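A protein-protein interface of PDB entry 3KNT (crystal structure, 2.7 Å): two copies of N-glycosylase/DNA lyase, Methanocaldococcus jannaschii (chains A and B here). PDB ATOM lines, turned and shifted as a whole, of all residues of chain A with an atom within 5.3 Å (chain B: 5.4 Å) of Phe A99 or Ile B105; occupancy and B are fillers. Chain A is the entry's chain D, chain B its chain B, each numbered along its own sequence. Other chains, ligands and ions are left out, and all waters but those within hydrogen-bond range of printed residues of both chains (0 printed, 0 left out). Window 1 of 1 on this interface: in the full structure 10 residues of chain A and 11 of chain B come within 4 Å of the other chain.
Phe A99 touches Ile B105, but with the chains exchanged Ile A105 does not touch Phe B99 (4.5 Å).
Asn B101 touches its own counterpart, Asn A101.
Phe A118 touches Phe B99, but with the chains exchanged Phe A99 does not touch Phe B118 (4.5 Å).
Positions printed for both chains: 99, 101, 102, 105 and 118.
O of Arg A98 sits at hydrogen-bond distance from ND2 of Asn B101, at 3.4 Å.
NH2 of Arg A98 is in hydrogen-bond range of OG of Ser B108 (2.8 Å).
The side-chain carboxylate (OD2) of Asp B104 is in salt-bridge range of the side-chain amino group (NZ) of Lys A100 (3.0 Å).
Phe A99 touches just one residue of chain B: Ile B105 (3.8 Å).
Of the printed residues of chain B, Lys A100 touches Asn B101 (3.6 Å) and Asp B104 (3.0 Å).
Printed residues of chain B within 4 Å of Asn A122: Phe B118 (3.6 Å).
Ile A123 touches none of the printed residues of chain B.
Printed residues of chain A within 4 Å of Phe B109: Arg A98.
Of the printed residues of chain A, Phe B118 touches Asn A122.
The nearest printed residue of chain A that does not touch Ile B105 is Ile A105 (5.4 Å).
The nearest printed residue of chain B that does not touch Phe A118 is Phe B118 (4.5 Å).
Printed residues of chain B that touch a printed residue of chain A: Phe B99, Asn B101, Asp B104, Ile B105, Ser B108, Phe B109 and Phe B118.
Hydrophobic or aromatic side chains of chain A within 4 Å of the printed part of chain B: Phe A99 and Phe A118.
Among the printed residues, Asp or Glu carboxylates within 4 Å of a Lys or Arg side-chain nitrogen of the other chain: Lys A100 with Asp B104 (3.0 Å).
Among the printed residues, pairs that only touch across the chains: Arg A98 with Asp B104 (3.9 Å), Arg A98 with Ile B105 (3.9 Å), Arg A98 with Phe B109 (3.9 Å), Phe A99 with Ile B105 (3.8 Å), Lys A100 with Asn B101 (3.6 Å), Asn A101 with Asn B101 (3.5 Å), Phe A118 with Phe B99 (3.97 Å) and Asn A122 with Phe B118 (3.6 Å).
O of Phe A118 is in hydrogen-bond range of ND2 of Asn A122 (2.9 Å).
OG of Ser B108 sits close to O of Asp B104 (3.3 Å).
OG of Ser B108 is in hydrogen-bond range of O of Ile B105, 2.6 Å away.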
ATOM      1  N   PHE A  38       3.122   2.055  13.320  1.00  0.00           N
ATOM      2  CA  PHE A  38       2.661   1.670  14.645  1.00  0.00           C
ATOM      3  C   PHE A  38       1.708   2.719  15.216  1.00  0.00           C
ATOM      4  O   PHE A  38       0.666   2.378  15.774  1.00  0.00           O
ATOM      5  CB  PHE A  38       3.849   1.440  15.584  1.00  0.00           C
ATOM      6  CG  PHE A  38       3.454   1.009  16.967  1.00  0.00           C
ATOM      7  CD1 PHE A  38       3.033  -0.288  17.211  1.00  0.00           C
ATOM      8  CD2 PHE A  38       3.507   1.901  18.023  1.00  0.00           C
ATOM      9  CE1 PHE A  38       2.670  -0.684  18.485  1.00  0.00           C
ATOM     10  CE2 PHE A  38       3.146   1.510  19.298  1.00  0.00           C
ATOM     11  CZ  PHE A  38       2.727   0.217  19.529  1.00  0.00           C
ATOM     12  N   ALA A  96       0.919  -4.123  22.714  1.00  0.00           N
ATOM     13  CA  ALA A  96       1.135  -4.226  21.275  1.00  0.00           C
ATOM     14  C   ALA A  96       2.595  -4.000  20.892  1.00  0.00           C
ATOM     15  O   ALA A  96       3.037  -4.430  19.828  1.00  0.00           O
ATOM     16  CB  ALA A  96       0.234  -3.253  20.531  1.00  0.00           C
ATOM     17  N   ARG A  97       3.339  -3.330  21.766  1.00  0.00           N
ATOM     18  CA  ARG A  97       4.724  -2.968  21.474  1.00  0.00           C
ATOM     19  C   ARG A  97       5.603  -4.161  21.103  1.00  0.00           C
ATOM     20  O   ARG A  97       6.677  -3.989  20.524  1.00  0.00           O
ATOM     21  CB  ARG A  97       5.332  -2.188  22.639  1.00  0.00           C
ATOM     22  CG  ARG A  97       4.850  -0.751  22.713  1.00  0.00           C
ATOM     23  CD  ARG A  97       5.228  -0.103  24.028  1.00  0.00           C
ATOM     24  NE  ARG A  97       4.926   1.325  24.030  1.00  0.00           N
ATOM     25  CZ  ARG A  97       4.915   2.085  25.120  1.00  0.00           C
ATOM     26  NH1 ARG A  97       5.184   1.552  26.303  1.00  0.00           N
ATOM     27  NH2 ARG A  97       4.629   3.376  25.025  1.00  0.00           N
ATOM     28  N   ARG A  98       5.149  -5.366  21.433  1.00  0.00           N
ATOM     29  CA  ARG A  98       5.858  -6.575  21.032  1.00  0.00           C
ATOM     30  C   ARG A  98       6.080  -6.581  19.522  1.00  0.00           C
ATOM     31  O   ARG A  98       7.081  -7.105  19.034  1.00  0.00           O
ATOM     32  CB  ARG A  98       5.083  -7.821  21.457  1.00  0.00           C
ATOM     33  CG  ARG A  98       3.587  -7.688  21.272  1.00  0.00           C
ATOM     34  CD  ARG A  98       2.937  -9.022  20.961  1.00  0.00           C
ATOM     35  NE  ARG A  98       2.969  -9.953  22.084  1.00  0.00           N
ATOM     36  CZ  ARG A  98       2.270 -11.081  22.125  1.00  0.00           C
ATOM     37  NH1 ARG A  98       1.486 -11.412  21.106  1.00  0.00           N
ATOM     38  NH2 ARG A  98       2.347 -11.878  23.181  1.00  0.00           N
ATOM     39  N   PHE A  99       5.141  -5.991  18.786  1.00  0.00           N
ATOM     40  CA  PHE A  99       5.257  -5.881  17.335  1.00  0.00           C
ATOM     41  C   PHE A  99       5.449  -4.435  16.898  1.00  0.00           C
ATOM     42  O   PHE A  99       4.732  -3.950  16.021  1.00  0.00           O
ATOM     43  CB  PHE A  99       4.015  -6.444  16.646  1.00  0.00           C
ATOM     44  CG  PHE A  99       3.663  -7.836  17.069  1.00  0.00           C
ATOM     45  CD1 PHE A  99       4.591  -8.858  16.971  1.00  0.00           C
ATOM     46  CD2 PHE A  99       2.399  -8.126  17.551  1.00  0.00           C
ATOM     47  CE1 PHE A  99       4.268 -10.142  17.358  1.00  0.00           C
ATOM     48  CE2 PHE A  99       2.069  -9.408  17.937  1.00  0.00           C
ATOM     49  CZ  PHE A  99       3.005 -10.417  17.843  1.00  0.00           C
ATOM     50  N   LYS A 100       6.412  -3.745  17.499  1.00  0.00           N
ATOM     51  CA  LYS A 100       6.647  -2.345  17.164  1.00  0.00           C
ATOM     52  C   LYS A 100       7.218  -2.190  15.756  1.00  0.00           C
ATOM     53  O   LYS A 100       7.145  -1.113  15.165  1.00  0.00           O
ATOM     54  CB  LYS A 100       7.544  -1.667  18.203  1.00  0.00           C
ATOM     55  CG  LYS A 100       8.969  -2.181  18.253  1.00  0.00           C
ATOM     56  CD  LYS A 100       9.759  -1.454  19.329  1.00  0.00           C
ATOM     57  CE  LYS A 100      11.216  -1.878  19.336  1.00  0.00           C
ATOM     58  NZ  LYS A 100      11.368  -3.337  19.587  1.00  0.00           N
ATOM     59  N   ASN A 101       7.780  -3.269  15.220  1.00  0.00           N
ATOM     60  CA  ASN A 101       8.200  -3.291  13.823  1.00  0.00           C
ATOM     61  C   ASN A 101       7.047  -3.754  12.944  1.00  0.00           C
ATOM     62  O   ASN A 101       7.188  -4.683  12.148  1.00  0.00           O
ATOM     63  CB  ASN A 101       9.412  -4.205  13.629  1.00  0.00           C
ATOM     64  CG  ASN A 101       9.141  -5.636  14.057  1.00  0.00           C
ATOM     65  OD1 ASN A 101       8.466  -5.881  15.055  1.00  0.00           O
ATOM     66  ND2 ASN A 101       9.672  -6.590  13.300  1.00  0.00           N
ATOM     67  N   ILE A 102       5.903  -3.098  13.098  1.00  0.00           N
ATOM     68  CA  ILE A 102       4.669  -3.536  12.456  1.00  0.00           C
ATOM     69  C   ILE A 102       4.727  -3.475  10.932  1.00  0.00           C
ATOM     70  O   ILE A 102       4.147  -4.320  10.252  1.00  0.00           O
ATOM     71  CB  ILE A 102       3.451  -2.731  12.968  1.00  0.00           C
ATOM     72  CG1 ILE A 102       2.149  -3.345  12.451  1.00  0.00           C
ATOM     73  CG2 ILE A 102       3.569  -1.265  12.576  1.00  0.00           C
ATOM     74  CD1 ILE A 102       1.947  -4.780  12.879  1.00  0.00           C
ATOM     75  N   ILE A 105       6.586  -6.535   9.671  1.00  0.00           N
ATOM     76  CA  ILE A 105       5.778  -7.722   9.914  1.00  0.00           C
ATOM     77  C   ILE A 105       4.642  -7.833   8.907  1.00  0.00           C
ATOM     78  O   ILE A 105       4.368  -8.910   8.383  1.00  0.00           O
ATOM     79  CB  ILE A 105       5.197  -7.728  11.335  1.00  0.00           C
ATOM     80  CG1 ILE A 105       6.296  -8.041  12.351  1.00  0.00           C
ATOM     81  CG2 ILE A 105       4.067  -8.737  11.444  1.00  0.00           C
ATOM     82  CD1 ILE A 105       5.786  -8.255  13.754  1.00  0.00           C
ATOM     83  N   PHE A 118      -3.674 -12.088  10.928  1.00  0.00           N
ATOM     84  CA  PHE A 118      -2.627 -12.162  11.939  1.00  0.00           C
ATOM     85  C   PHE A 118      -2.824 -11.133  13.048  1.00  0.00           C
ATOM     86  O   PHE A 118      -2.644 -11.436  14.227  1.00  0.00           O
ATOM     87  CB  PHE A 118      -1.256 -11.969  11.289  1.00  0.00           C
ATOM     88  CG  PHE A 118      -0.106 -12.099  12.245  1.00  0.00           C
ATOM     89  CD1 PHE A 118       0.429 -10.983  12.864  1.00  0.00           C
ATOM     90  CD2 PHE A 118       0.440 -13.341  12.520  1.00  0.00           C
ATOM     91  CE1 PHE A 118       1.486 -11.102  13.742  1.00  0.00           C
ATOM     92  CE2 PHE A 118       1.499 -13.467  13.398  1.00  0.00           C
ATOM     93  CZ  PHE A 118       2.022 -12.346  14.010  1.00  0.00           C
ATOM     94  N   ASN A 122      -3.618 -11.900  17.161  1.00  0.00           N
ATOM     95  CA  ASN A 122      -2.372 -11.602  17.870  1.00  0.00           C
ATOM     96  C   ASN A 122      -2.316 -10.213  18.512  1.00  0.00           C
ATOM     97  O   ASN A 122      -1.370  -9.876  19.225  1.00  0.00           O
ATOM     98  CB  ASN A 122      -1.177 -11.795  16.953  1.00  0.00           C
ATOM     99  CG  ASN A 122      -0.957 -13.244  16.596  1.00  0.00           C
ATOM    100  OD1 ASN A 122      -0.749 -14.089  17.466  1.00  0.00           O
ATOM    101  ND2 ASN A 122      -0.993 -13.542  15.310  1.00  0.00           N
ATOM    102  N   ILE A 123      -3.320  -9.391  18.261  1.00  0.00           N
ATOM    103  CA  ILE A 123      -3.374  -8.135  18.977  1.00  0.00           C
ATOM    104  C   ILE A 123      -4.700  -7.986  19.715  1.00  0.00           C
ATOM    105  O   ILE A 123      -5.781  -7.974  19.102  1.00  0.00           O
ATOM    106  CB  ILE A 123      -3.036  -6.939  18.071  1.00  0.00           C
ATOM    107  CG1 ILE A 123      -1.701  -7.193  17.375  1.00  0.00           C
ATOM    108  CG2 ILE A 123      -2.934  -5.647  18.881  1.00  0.00           C
ATOM    109  CD1 ILE A 123      -1.139  -5.981  16.673  1.00  0.00           C
ATOM    110  N   PHE B  99      10.160 -11.693  12.688  1.00  0.00           N
ATOM    111  CA  PHE B  99      10.175 -11.643  14.144  1.00  0.00           C
ATOM    112  C   PHE B  99      11.600 -11.422  14.635  1.00  0.00           C
ATOM    113  O   PHE B  99      12.033 -12.040  15.607  1.00  0.00           O
ATOM    114  CB  PHE B  99       9.622 -12.937  14.739  1.00  0.00           C
ATOM    115  CG  PHE B  99       8.279 -13.328  14.198  1.00  0.00           C
ATOM    116  CD1 PHE B  99       7.192 -12.480  14.326  1.00  0.00           C
ATOM    117  CD2 PHE B  99       8.100 -14.549  13.569  1.00  0.00           C
ATOM    118  CE1 PHE B  99       5.955 -12.838  13.829  1.00  0.00           C
ATOM    119  CE2 PHE B  99       6.864 -14.913  13.071  1.00  0.00           C
ATOM    120  CZ  PHE B  99       5.791 -14.056  13.203  1.00  0.00           C
ATOM    121  N   ASN B 101      12.886  -9.371  16.354  1.00  0.00           N
ATOM    122  CA  ASN B 101      12.916  -9.087  17.785  1.00  0.00           C
ATOM    123  C   ASN B 101      12.159 -10.164  18.560  1.00  0.00           C
ATOM    124  O   ASN B 101      11.105  -9.904  19.145  1.00  0.00           O
ATOM    125  CB  ASN B 101      12.354  -7.695  18.088  1.00  0.00           C
ATOM    126  CG  ASN B 101      10.928  -7.518  17.597  1.00  0.00           C
ATOM    127  OD1 ASN B 101      10.405  -8.347  16.856  1.00  0.00           O
ATOM    128  ND2 ASN B 101      10.294  -6.428  18.012  1.00  0.00           N
ATOM    129  N   ILE B 102      12.715 -11.372  18.556  1.00  0.00           N
ATOM    130  CA  ILE B 102      12.043 -12.541  19.117  1.00  0.00           C
ATOM    131  C   ILE B 102      11.962 -12.517  20.644  1.00  0.00           C
ATOM    132  O   ILE B 102      11.280 -13.346  21.246  1.00  0.00           O
ATOM    133  CB  ILE B 102      12.721 -13.850  18.654  1.00  0.00           C
ATOM    134  CG1 ILE B 102      11.861 -15.065  19.010  1.00  0.00           C
ATOM    135  CG2 ILE B 102      14.115 -13.971  19.253  1.00  0.00           C
ATOM    136  CD1 ILE B 102      10.468 -15.020  18.418  1.00  0.00           C
ATOM    137  N   LYS B 103      12.649 -11.569  21.272  1.00  0.00           N
ATOM    138  CA  LYS B 103      12.622 -11.468  22.728  1.00  0.00           C
ATOM    139  C   LYS B 103      11.372 -10.744  23.221  1.00  0.00           C
ATOM    140  O   LYS B 103      10.694 -11.216  24.136  1.00  0.00           O
ATOM    141  CB  LYS B 103      13.883 -10.786  23.259  1.00  0.00           C
ATOM    142  CG  LYS B 103      13.981 -10.793  24.775  1.00  0.00           C
ATOM    143  CD  LYS B 103      15.351 -10.345  25.254  1.00  0.00           C
ATOM    144  CE  LYS B 103      15.463 -10.471  26.764  1.00  0.00           C
ATOM    145  NZ  LYS B 103      16.808 -10.084  27.266  1.00  0.00           N
ATOM    146  N   ASP B 104      11.072  -9.596  22.618  1.00  0.00           N
ATOM    147  CA  ASP B 104       9.859  -8.856  22.944  1.00  0.00           C
ATOM    148  C   ASP B 104       8.641  -9.762  22.822  1.00  0.00           C
ATOM    149  O   ASP B 104       7.710  -9.685  23.621  1.00  0.00           O
ATOM    150  CB  ASP B 104       9.691  -7.656  22.010  1.00  0.00           C
ATOM    151  CG  ASP B 104      10.696  -6.555  22.281  1.00  0.00           C
ATOM    152  OD1 ASP B 104      11.528  -6.718  23.198  1.00  0.00           O
ATOM    153  OD2 ASP B 104      10.652  -5.523  21.576  1.00  0.00           O
ATOM    154  N   ILE B 105       8.663 -10.623  21.810  1.00  0.00           N
ATOM    155  CA  ILE B 105       7.534 -11.491  21.505  1.00  0.00           C
ATOM    156  C   ILE B 105       7.402 -12.642  22.500  1.00  0.00           C
ATOM    157  O   ILE B 105       6.295 -13.008  22.893  1.00  0.00           O
ATOM    158  CB  ILE B 105       7.644 -12.061  20.078  1.00  0.00           C
ATOM    159  CG1 ILE B 105       7.658 -10.925  19.052  1.00  0.00           C
ATOM    160  CG2 ILE B 105       6.506 -13.030  19.797  1.00  0.00           C
ATOM    161  CD1 ILE B 105       7.808 -11.393  17.622  1.00  0.00           C
ATOM    162  N   VAL B 106       8.534 -13.210  22.905  1.00  0.00           N
ATOM    163  CA  VAL B 106       8.527 -14.374  23.787  1.00  0.00           C
ATOM    164  C   VAL B 106       8.251 -14.022  25.248  1.00  0.00           C
ATOM    165  O   VAL B 106       7.454 -14.686  25.911  1.00  0.00           O
ATOM    166  CB  VAL B 106       9.843 -15.177  23.679  1.00  0.00           C
ATOM    167  CG1 VAL B 106       9.940 -16.199  24.799  1.00  0.00           C
ATOM    168  CG2 VAL B 106       9.930 -15.863  22.326  1.00  0.00           C
ATOM    169  N   GLU B 107       8.903 -12.977  25.747  1.00  0.00           N
ATOM    170  CA  GLU B 107       8.749 -12.585  27.147  1.00  0.00           C
ATOM    171  C   GLU B 107       7.393 -11.948  27.432  1.00  0.00           C
ATOM    172  O   GLU B 107       6.998 -11.806  28.590  1.00  0.00           O
ATOM    173  CB  GLU B 107       9.876 -11.643  27.575  1.00  0.00           C
ATOM    174  CG  GLU B 107      11.238 -12.313  27.660  1.00  0.00           C
ATOM    175  CD  GLU B 107      12.265 -11.461  28.378  1.00  0.00           C
ATOM    176  OE1 GLU B 107      11.978 -10.275  28.641  1.00  0.00           O
ATOM    177  OE2 GLU B 107      13.360 -11.981  28.680  1.00  0.00           O
ATOM    178  N   SER B 108       6.686 -11.565  26.374  1.00  0.00           N
ATOM    179  CA  SER B 108       5.371 -10.954  26.517  1.00  0.00           C
ATOM    180  C   SER B 108       4.338 -11.985  26.955  1.00  0.00           C
ATOM    181  O   SER B 108       3.360 -11.654  27.625  1.00  0.00           O
ATOM    182  CB  SER B 108       4.938 -10.302  25.204  1.00  0.00           C
ATOM    183  OG  SER B 108       4.869 -11.260  24.162  1.00  0.00           O
ATOM    184  N   PHE B 109       4.560 -13.237  26.571  1.00  0.00           N
ATOM    185  CA  PHE B 109       3.673 -14.324  26.962  1.00  0.00           C
ATOM    186  C   PHE B 109       3.731 -14.569  28.462  1.00  0.00           C
ATOM    187  O   PHE B 109       4.730 -14.266  29.114  1.00  0.00           O
ATOM    188  CB  PHE B 109       4.024 -15.609  26.212  1.00  0.00           C
ATOM    189  CG  PHE B 109       3.643 -15.585  24.762  1.00  0.00           C
ATOM    190  CD1 PHE B 109       2.323 -15.749  24.379  1.00  0.00           C
ATOM    191  CD2 PHE B 109       4.603 -15.404  23.785  1.00  0.00           C
ATOM    192  CE1 PHE B 109       1.969 -15.729  23.048  1.00  0.00           C
ATOM    193  CE2 PHE B 109       4.256 -15.383  22.451  1.00  0.00           C
ATOM    194  CZ  PHE B 109       2.935 -15.544  22.081  1.00  0.00           C
ATOM    195  N   PHE B 118       2.991 -20.370  20.374  1.00  0.00           N
ATOM    196  CA  PHE B 118       3.075 -19.330  19.362  1.00  0.00           C
ATOM    197  C   PHE B 118       4.162 -19.648  18.345  1.00  0.00           C
ATOM    198  O   PHE B 118       3.884 -19.824  17.159  1.00  0.00           O
ATOM    199  CB  PHE B 118       3.366 -17.981  20.015  1.00  0.00           C
ATOM    200  CG  PHE B 118       3.569 -16.866  19.033  1.00  0.00           C
ATOM    201  CD1 PHE B 118       4.802 -16.666  18.437  1.00  0.00           C
ATOM    202  CD2 PHE B 118       2.525 -16.018  18.705  1.00  0.00           C
ATOM    203  CE1 PHE B 118       4.993 -15.642  17.531  1.00  0.00           C
ATOM    204  CE2 PHE B 118       2.709 -14.991  17.800  1.00  0.00           C
ATOM    205  CZ  PHE B 118       3.945 -14.803  17.213  1.00  0.00           C
